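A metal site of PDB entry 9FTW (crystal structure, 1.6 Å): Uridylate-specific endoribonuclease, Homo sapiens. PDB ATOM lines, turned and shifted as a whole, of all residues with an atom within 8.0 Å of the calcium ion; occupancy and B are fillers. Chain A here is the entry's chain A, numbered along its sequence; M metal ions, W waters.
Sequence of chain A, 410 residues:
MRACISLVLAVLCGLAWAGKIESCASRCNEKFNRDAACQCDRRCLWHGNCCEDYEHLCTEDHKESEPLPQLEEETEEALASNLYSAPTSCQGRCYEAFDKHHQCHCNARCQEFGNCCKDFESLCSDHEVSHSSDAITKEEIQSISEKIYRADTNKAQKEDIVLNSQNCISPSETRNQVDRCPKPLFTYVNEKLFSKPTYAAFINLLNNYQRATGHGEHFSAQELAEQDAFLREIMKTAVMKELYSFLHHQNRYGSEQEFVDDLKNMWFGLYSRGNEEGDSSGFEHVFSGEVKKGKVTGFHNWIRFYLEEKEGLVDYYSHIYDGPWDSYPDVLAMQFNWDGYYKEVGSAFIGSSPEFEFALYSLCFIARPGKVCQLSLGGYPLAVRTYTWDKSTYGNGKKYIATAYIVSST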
ATOM      1  N   GLN A 166       1.365 -25.565  21.894  1.00  0.00           N
ATOM      2  CA  GLN A 166       1.665 -24.360  22.677  1.00  0.00           C
ATOM      3  C   GLN A 166       0.584 -23.252  22.516  1.00  0.00           C
ATOM      4  O   GLN A 166      -0.594 -23.561  22.663  1.00  0.00           O
ATOM      5  CB  GLN A 166       3.112 -23.880  22.351  1.00  0.00           C
ATOM      6  CG  GLN A 166       4.183 -24.896  22.742  1.00  0.00           C
ATOM      7  CD  GLN A 166       5.468 -24.565  22.068  1.00  0.00           C
ATOM      8  OE1 GLN A 166       6.247 -23.734  22.577  1.00  0.00           O
ATOM      9  NE2 GLN A 166       5.706 -25.181  20.906  1.00  0.00           N
ATOM     10  N   VAL A 178       4.814 -12.458  15.794  1.00  0.00           N
ATOM     11  CA  VAL A 178       5.385 -12.542  17.134  1.00  0.00           C
ATOM     12  C   VAL A 178       5.497 -14.041  17.421  1.00  0.00           C
ATOM     13  O   VAL A 178       4.511 -14.772  17.286  1.00  0.00           O
ATOM     14  CB  VAL A 178       4.536 -11.835  18.229  1.00  0.00           C
ATOM     15  CG1 VAL A 178       5.077 -12.180  19.624  1.00  0.00           C
ATOM     16  CG2 VAL A 178       4.500 -10.308  18.033  1.00  0.00           C
ATOM     17  N   ASP A 179       6.693 -14.521  17.760  1.00  0.00           N
ATOM     18  CA  ASP A 179       6.875 -15.916  18.109  1.00  0.00           C
ATOM     19  C   ASP A 179       6.354 -16.107  19.541  1.00  0.00           C
ATOM     20  O   ASP A 179       6.936 -15.565  20.477  1.00  0.00           O
ATOM     21  CB  ASP A 179       8.354 -16.295  18.018  1.00  0.00           C
ATOM     22  CG  ASP A 179       8.628 -17.780  18.245  1.00  0.00           C
ATOM     23  OD1 ASP A 179       7.672 -18.517  18.556  1.00  0.00           O
ATOM     24  OD2 ASP A 179       9.800 -18.184  18.104  1.00  0.00           O
ATOM     25  N   ARG A 180       5.236 -16.816  19.680  1.00  0.00           N
ATOM     26  CA  ARG A 180       4.613 -17.110  20.981  1.00  0.00           C
ATOM     27  C   ARG A 180       4.831 -18.574  21.400  1.00  0.00           C
ATOM     28  O   ARG A 180       4.249 -19.004  22.409  1.00  0.00           O
ATOM     29  CB  ARG A 180       3.103 -16.789  20.904  1.00  0.00           C
ATOM     30  CG  ARG A 180       2.806 -15.334  21.201  1.00  0.00           C
ATOM     31  CD  ARG A 180       1.785 -14.653  20.345  1.00  0.00           C
ATOM     32  NE  ARG A 180       1.715 -13.223  20.693  1.00  0.00           N
ATOM     33  CZ  ARG A 180       1.018 -12.299  20.037  1.00  0.00           C
ATOM     34  NH1 ARG A 180       0.294 -12.642  18.964  1.00  0.00           N
ATOM     35  NH2 ARG A 180       1.027 -11.038  20.439  1.00  0.00           N
ATOM     36  N   CYS A 181       5.714 -19.317  20.710  1.00  0.00           N
ATOM     37  CA  CYS A 181       5.937 -20.729  20.987  1.00  0.00           C
ATOM     38  C   CYS A 181       7.440 -20.956  21.071  1.00  0.00           C
ATOM     39  O   CYS A 181       8.082 -21.128  20.031  1.00  0.00           O
ATOM     40  CB  CYS A 181       5.297 -21.573  19.886  1.00  0.00           C
ATOM     41  SG  CYS A 181       3.500 -21.378  19.783  1.00  0.00           S
ATOM     42  N   PRO A 182       8.029 -20.924  22.286  1.00  0.00           N
ATOM     43  CA  PRO A 182       9.502 -21.036  22.371  1.00  0.00           C
ATOM     44  C   PRO A 182      10.081 -22.412  22.052  1.00  0.00           C
ATOM     45  O   PRO A 182      11.272 -22.475  21.764  1.00  0.00           O
ATOM     46  CB  PRO A 182       9.826 -20.610  23.799  1.00  0.00           C
ATOM     47  CG  PRO A 182       8.601 -20.833  24.565  1.00  0.00           C
ATOM     48  CD  PRO A 182       7.426 -20.692  23.612  1.00  0.00           C
ATOM     49  N   LYS A 183       9.239 -23.468  22.073  1.00  0.00           N
ATOM     50  CA  LYS A 183       9.667 -24.830  21.805  1.00  0.00           C
ATOM     51  C   LYS A 183       9.287 -25.246  20.388  1.00  0.00           C
ATOM     52  O   LYS A 183       8.340 -24.677  19.813  1.00  0.00           O
ATOM     53  CB  LYS A 183       9.018 -25.779  22.839  1.00  0.00           C
ATOM     54  CG  LYS A 183       9.509 -25.579  24.287  1.00  0.00           C
ATOM     55  CD  LYS A 183      10.937 -26.078  24.511  1.00  0.00           C
ATOM     56  CE  LYS A 183      11.301 -26.115  25.982  1.00  0.00           C
ATOM     57  NZ  LYS A 183      11.291 -24.762  26.612  1.00  0.00           N
ATOM     58  N   PRO A 184       9.973 -26.233  19.785  1.00  0.00           N
ATOM     59  CA  PRO A 184       9.530 -26.693  18.452  1.00  0.00           C
ATOM     60  C   PRO A 184       8.117 -27.269  18.498  1.00  0.00           C
ATOM     61  O   PRO A 184       7.661 -27.753  19.552  1.00  0.00           O
ATOM     62  CB  PRO A 184      10.532 -27.800  18.083  1.00  0.00           C
ATOM     63  CG  PRO A 184      11.095 -28.266  19.396  1.00  0.00           C
ATOM     64  CD  PRO A 184      11.127 -27.028  20.274  1.00  0.00           C
ATOM     65  N   LEU A 185       7.417 -27.231  17.364  1.00  0.00           N
ATOM     66  CA  LEU A 185       6.086 -27.844  17.280  1.00  0.00           C
ATOM     67  C   LEU A 185       6.222 -29.375  17.416  1.00  0.00           C
ATOM     68  O   LEU A 185       5.403 -30.023  18.063  1.00  0.00           O
ATOM     69  CB  LEU A 185       5.426 -27.511  15.935  1.00  0.00           C
ATOM     70  CG  LEU A 185       4.111 -28.248  15.604  1.00  0.00           C
ATOM     71  CD1 LEU A 185       3.031 -27.960  16.654  1.00  0.00           C
ATOM     72  CD2 LEU A 185       3.629 -27.863  14.207  1.00  0.00           C
ATOM     73  N   GLU A 309      12.214 -27.697  10.416  1.00  0.00           N
ATOM     74  CA  GLU A 309      12.302 -27.259  11.833  1.00  0.00           C
ATOM     75  C   GLU A 309      13.511 -27.935  12.501  1.00  0.00           C
ATOM     76  O   GLU A 309      14.260 -27.304  13.233  1.00  0.00           O
ATOM     77  CB  GLU A 309      11.020 -27.625  12.573  1.00  0.00           C
ATOM     78  CG  GLU A 309      11.005 -27.206  14.025  1.00  0.00           C
ATOM     79  CD  GLU A 309       9.687 -27.512  14.699  1.00  0.00           C
ATOM     80  OE1 GLU A 309       9.297 -28.706  14.737  1.00  0.00           O
ATOM     81  OE2 GLU A 309       9.032 -26.552  15.162  1.00  0.00           O
ATOM     82  N   VAL A 314      12.775 -23.626   9.981  1.00  0.00           N
ATOM     83  CA  VAL A 314      11.397 -23.234  10.226  1.00  0.00           C
ATOM     84  C   VAL A 314      11.345 -22.925  11.724  1.00  0.00           C
ATOM     85  O   VAL A 314      11.868 -23.700  12.517  1.00  0.00           O
ATOM     86  CB  VAL A 314      10.391 -24.379   9.819  1.00  0.00           C
ATOM     87  CG1 VAL A 314       9.090 -24.292  10.634  1.00  0.00           C
ATOM     88  CG2 VAL A 314      10.083 -24.312   8.327  1.00  0.00           C
ATOM     89  N   ASP A 315      10.694 -21.817  12.100  1.00  0.00           N
ATOM     90  CA  ASP A 315      10.502 -21.451  13.488  1.00  0.00           C
ATOM     91  C   ASP A 315       9.005 -21.309  13.662  1.00  0.00           C
ATOM     92  O   ASP A 315       8.394 -20.424  13.077  1.00  0.00           O
ATOM     93  CB  ASP A 315      11.231 -20.154  13.845  1.00  0.00           C
ATOM     94  CG  ASP A 315      11.235 -19.805  15.317  1.00  0.00           C
ATOM     95  OD1 ASP A 315      10.445 -20.431  16.080  1.00  0.00           O
ATOM     96  OD2 ASP A 315      11.980 -18.875  15.705  1.00  0.00           O
ATOM     97  N   TYR A 316       8.410 -22.200  14.461  1.00  0.00           N
ATOM     98  CA  TYR A 316       6.972 -22.242  14.725  1.00  0.00           C
ATOM     99  C   TYR A 316       6.628 -21.049  15.612  1.00  0.00           C
ATOM    100  O   TYR A 316       7.248 -20.892  16.654  1.00  0.00           O
ATOM    101  CB  TYR A 316       6.656 -23.555  15.481  1.00  0.00           C
ATOM    102  CG  TYR A 316       5.235 -23.700  15.968  1.00  0.00           C
ATOM    103  CD1 TYR A 316       4.162 -23.591  15.100  1.00  0.00           C
ATOM    104  CD2 TYR A 316       4.974 -24.033  17.288  1.00  0.00           C
ATOM    105  CE1 TYR A 316       2.848 -23.744  15.543  1.00  0.00           C
ATOM    106  CE2 TYR A 316       3.671 -24.162  17.757  1.00  0.00           C
ATOM    107  CZ  TYR A 316       2.616 -24.075  16.870  1.00  0.00           C
ATOM    108  OH  TYR A 316       1.319 -24.240  17.291  1.00  0.00           O
ATOM    109  N   TYR A 317       5.630 -20.226  15.228  1.00  0.00           N
ATOM    110  CA  TYR A 317       5.281 -19.053  16.030  1.00  0.00           C
ATOM    111  C   TYR A 317       4.006 -19.233  16.852  1.00  0.00           C
ATOM    112  O   TYR A 317       3.882 -18.572  17.898  1.00  0.00           O
ATOM    113  CB  TYR A 317       5.053 -17.821  15.118  1.00  0.00           C
ATOM    114  CG  TYR A 317       6.296 -17.055  14.708  1.00  0.00           C
ATOM    115  CD1 TYR A 317       7.530 -17.682  14.621  1.00  0.00           C
ATOM    116  CD2 TYR A 317       6.216 -15.739  14.281  1.00  0.00           C
ATOM    117  CE1 TYR A 317       8.676 -16.992  14.243  1.00  0.00           C
ATOM    118  CE2 TYR A 317       7.360 -15.028  13.903  1.00  0.00           C
ATOM    119  CZ  TYR A 317       8.584 -15.668  13.854  1.00  0.00           C
ATOM    120  OH  TYR A 317       9.713 -15.012  13.430  1.00  0.00           O
ATOM    121  N   SER A 318       3.013 -19.918  16.292  1.00  0.00           N
ATOM    122  CA  SER A 318       1.700 -20.085  16.953  1.00  0.00           C
ATOM    123  C   SER A 318       0.748 -20.888  16.023  1.00  0.00           C
ATOM    124  O   SER A 318       1.105 -21.201  14.882  1.00  0.00           O
ATOM    125  CB  SER A 318       1.080 -18.699  17.265  1.00  0.00           C
ATOM    126  OG  SER A 318       1.001 -17.832  16.134  1.00  0.00           O
ATOM    127  N   GLN A 335       1.270 -20.409  12.147  1.00  0.00           N
ATOM    128  CA  GLN A 335       2.056 -19.222  11.817  1.00  0.00           C
ATOM    129  C   GLN A 335       3.515 -19.648  11.990  1.00  0.00           C
ATOM    130  O   GLN A 335       3.839 -20.285  13.010  1.00  0.00           O
ATOM    131  CB  GLN A 335       1.789 -18.082  12.814  1.00  0.00           C
ATOM    132  CG  GLN A 335       0.428 -17.434  12.721  1.00  0.00           C
ATOM    133  CD  GLN A 335      -0.686 -18.395  13.051  1.00  0.00           C
ATOM    134  OE1 GLN A 335      -0.829 -18.822  14.200  1.00  0.00           O
ATOM    135  NE2 GLN A 335      -1.468 -18.768  12.046  1.00  0.00           N
ATOM    136  N   PHE A 336       4.398 -19.346  11.015  1.00  0.00           N
ATOM    137  CA  PHE A 336       5.798 -19.714  11.162  1.00  0.00           C
ATOM    138  C   PHE A 336       6.715 -18.889  10.278  1.00  0.00           C
ATOM    139  O   PHE A 336       6.249 -18.278   9.319  1.00  0.00           O
ATOM    140  CB  PHE A 336       5.997 -21.219  10.930  1.00  0.00           C
ATOM    141  CG  PHE A 336       5.547 -21.755   9.600  1.00  0.00           C
ATOM    142  CD1 PHE A 336       4.245 -22.189   9.408  1.00  0.00           C
ATOM    143  CD2 PHE A 336       6.433 -21.849   8.527  1.00  0.00           C
ATOM    144  CE1 PHE A 336       3.854 -22.764   8.211  1.00  0.00           C
ATOM    145  CE2 PHE A 336       6.041 -22.433   7.334  1.00  0.00           C
ATOM    146  CZ  PHE A 336       4.751 -22.875   7.174  1.00  0.00           C
ATOM    147  N   ASN A 337       8.014 -18.829  10.639  1.00  0.00           N
ATOM    148  CA  ASN A 337       9.031 -18.149   9.839  1.00  0.00           C
ATOM    149  C   ASN A 337       9.838 -19.247   9.168  1.00  0.00           C
ATOM    150  O   ASN A 337      10.252 -20.188   9.836  1.00  0.00           O
ATOM    151  CB  ASN A 337       9.949 -17.295  10.731  1.00  0.00           C
ATOM    152  CG  ASN A 337      10.965 -16.498   9.941  1.00  0.00           C
ATOM    153  OD1 ASN A 337      12.001 -17.018   9.500  1.00  0.00           O
ATOM    154  ND2 ASN A 337      10.721 -15.203   9.764  1.00  0.00           N
HETATM  155 CA    CA M   1       9.154 -20.431  18.009  1.00  0.00          CA
HETATM  156  O   HOH W   1      11.301 -20.479  19.296  1.00  0.00           O
HETATM  157  O   HOH W   2       9.474 -22.826  18.032  1.00  0.00           O
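O of Asn 337 is in hydrogen-bond range of N of Asp 315, at 2.8 Å. SG of Cys 181 is in hydrogen-bond range of O of Tyr 317 (3.4 Å).
Four residues have an atom within 4 Å of the calcium ion: Asp 179, Cys 181, Asp 315 and Tyr 316. The nearest printed residue that does not touch the calcium ion is Pro 182 (4.4 Å).
The calcium ion is bound by the side-chain carboxylate (OD1) of Asp 315 (2.3 Å), the side-chain carboxylate (OD2) of Asp 179 (2.3 Å), the backbone carbonyl oxygen (O) of Tyr 316 (2.4 Å), the backbone carbonyl oxygen (O) of Cys 181 (2.4 Å), water W2 (2.4 Å), the side-chain carboxylate (OD1) of Asp 179 (2.5 Å) and water W1 (2.5 Å). The calcium ion has seven donor atoms within binding distance.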
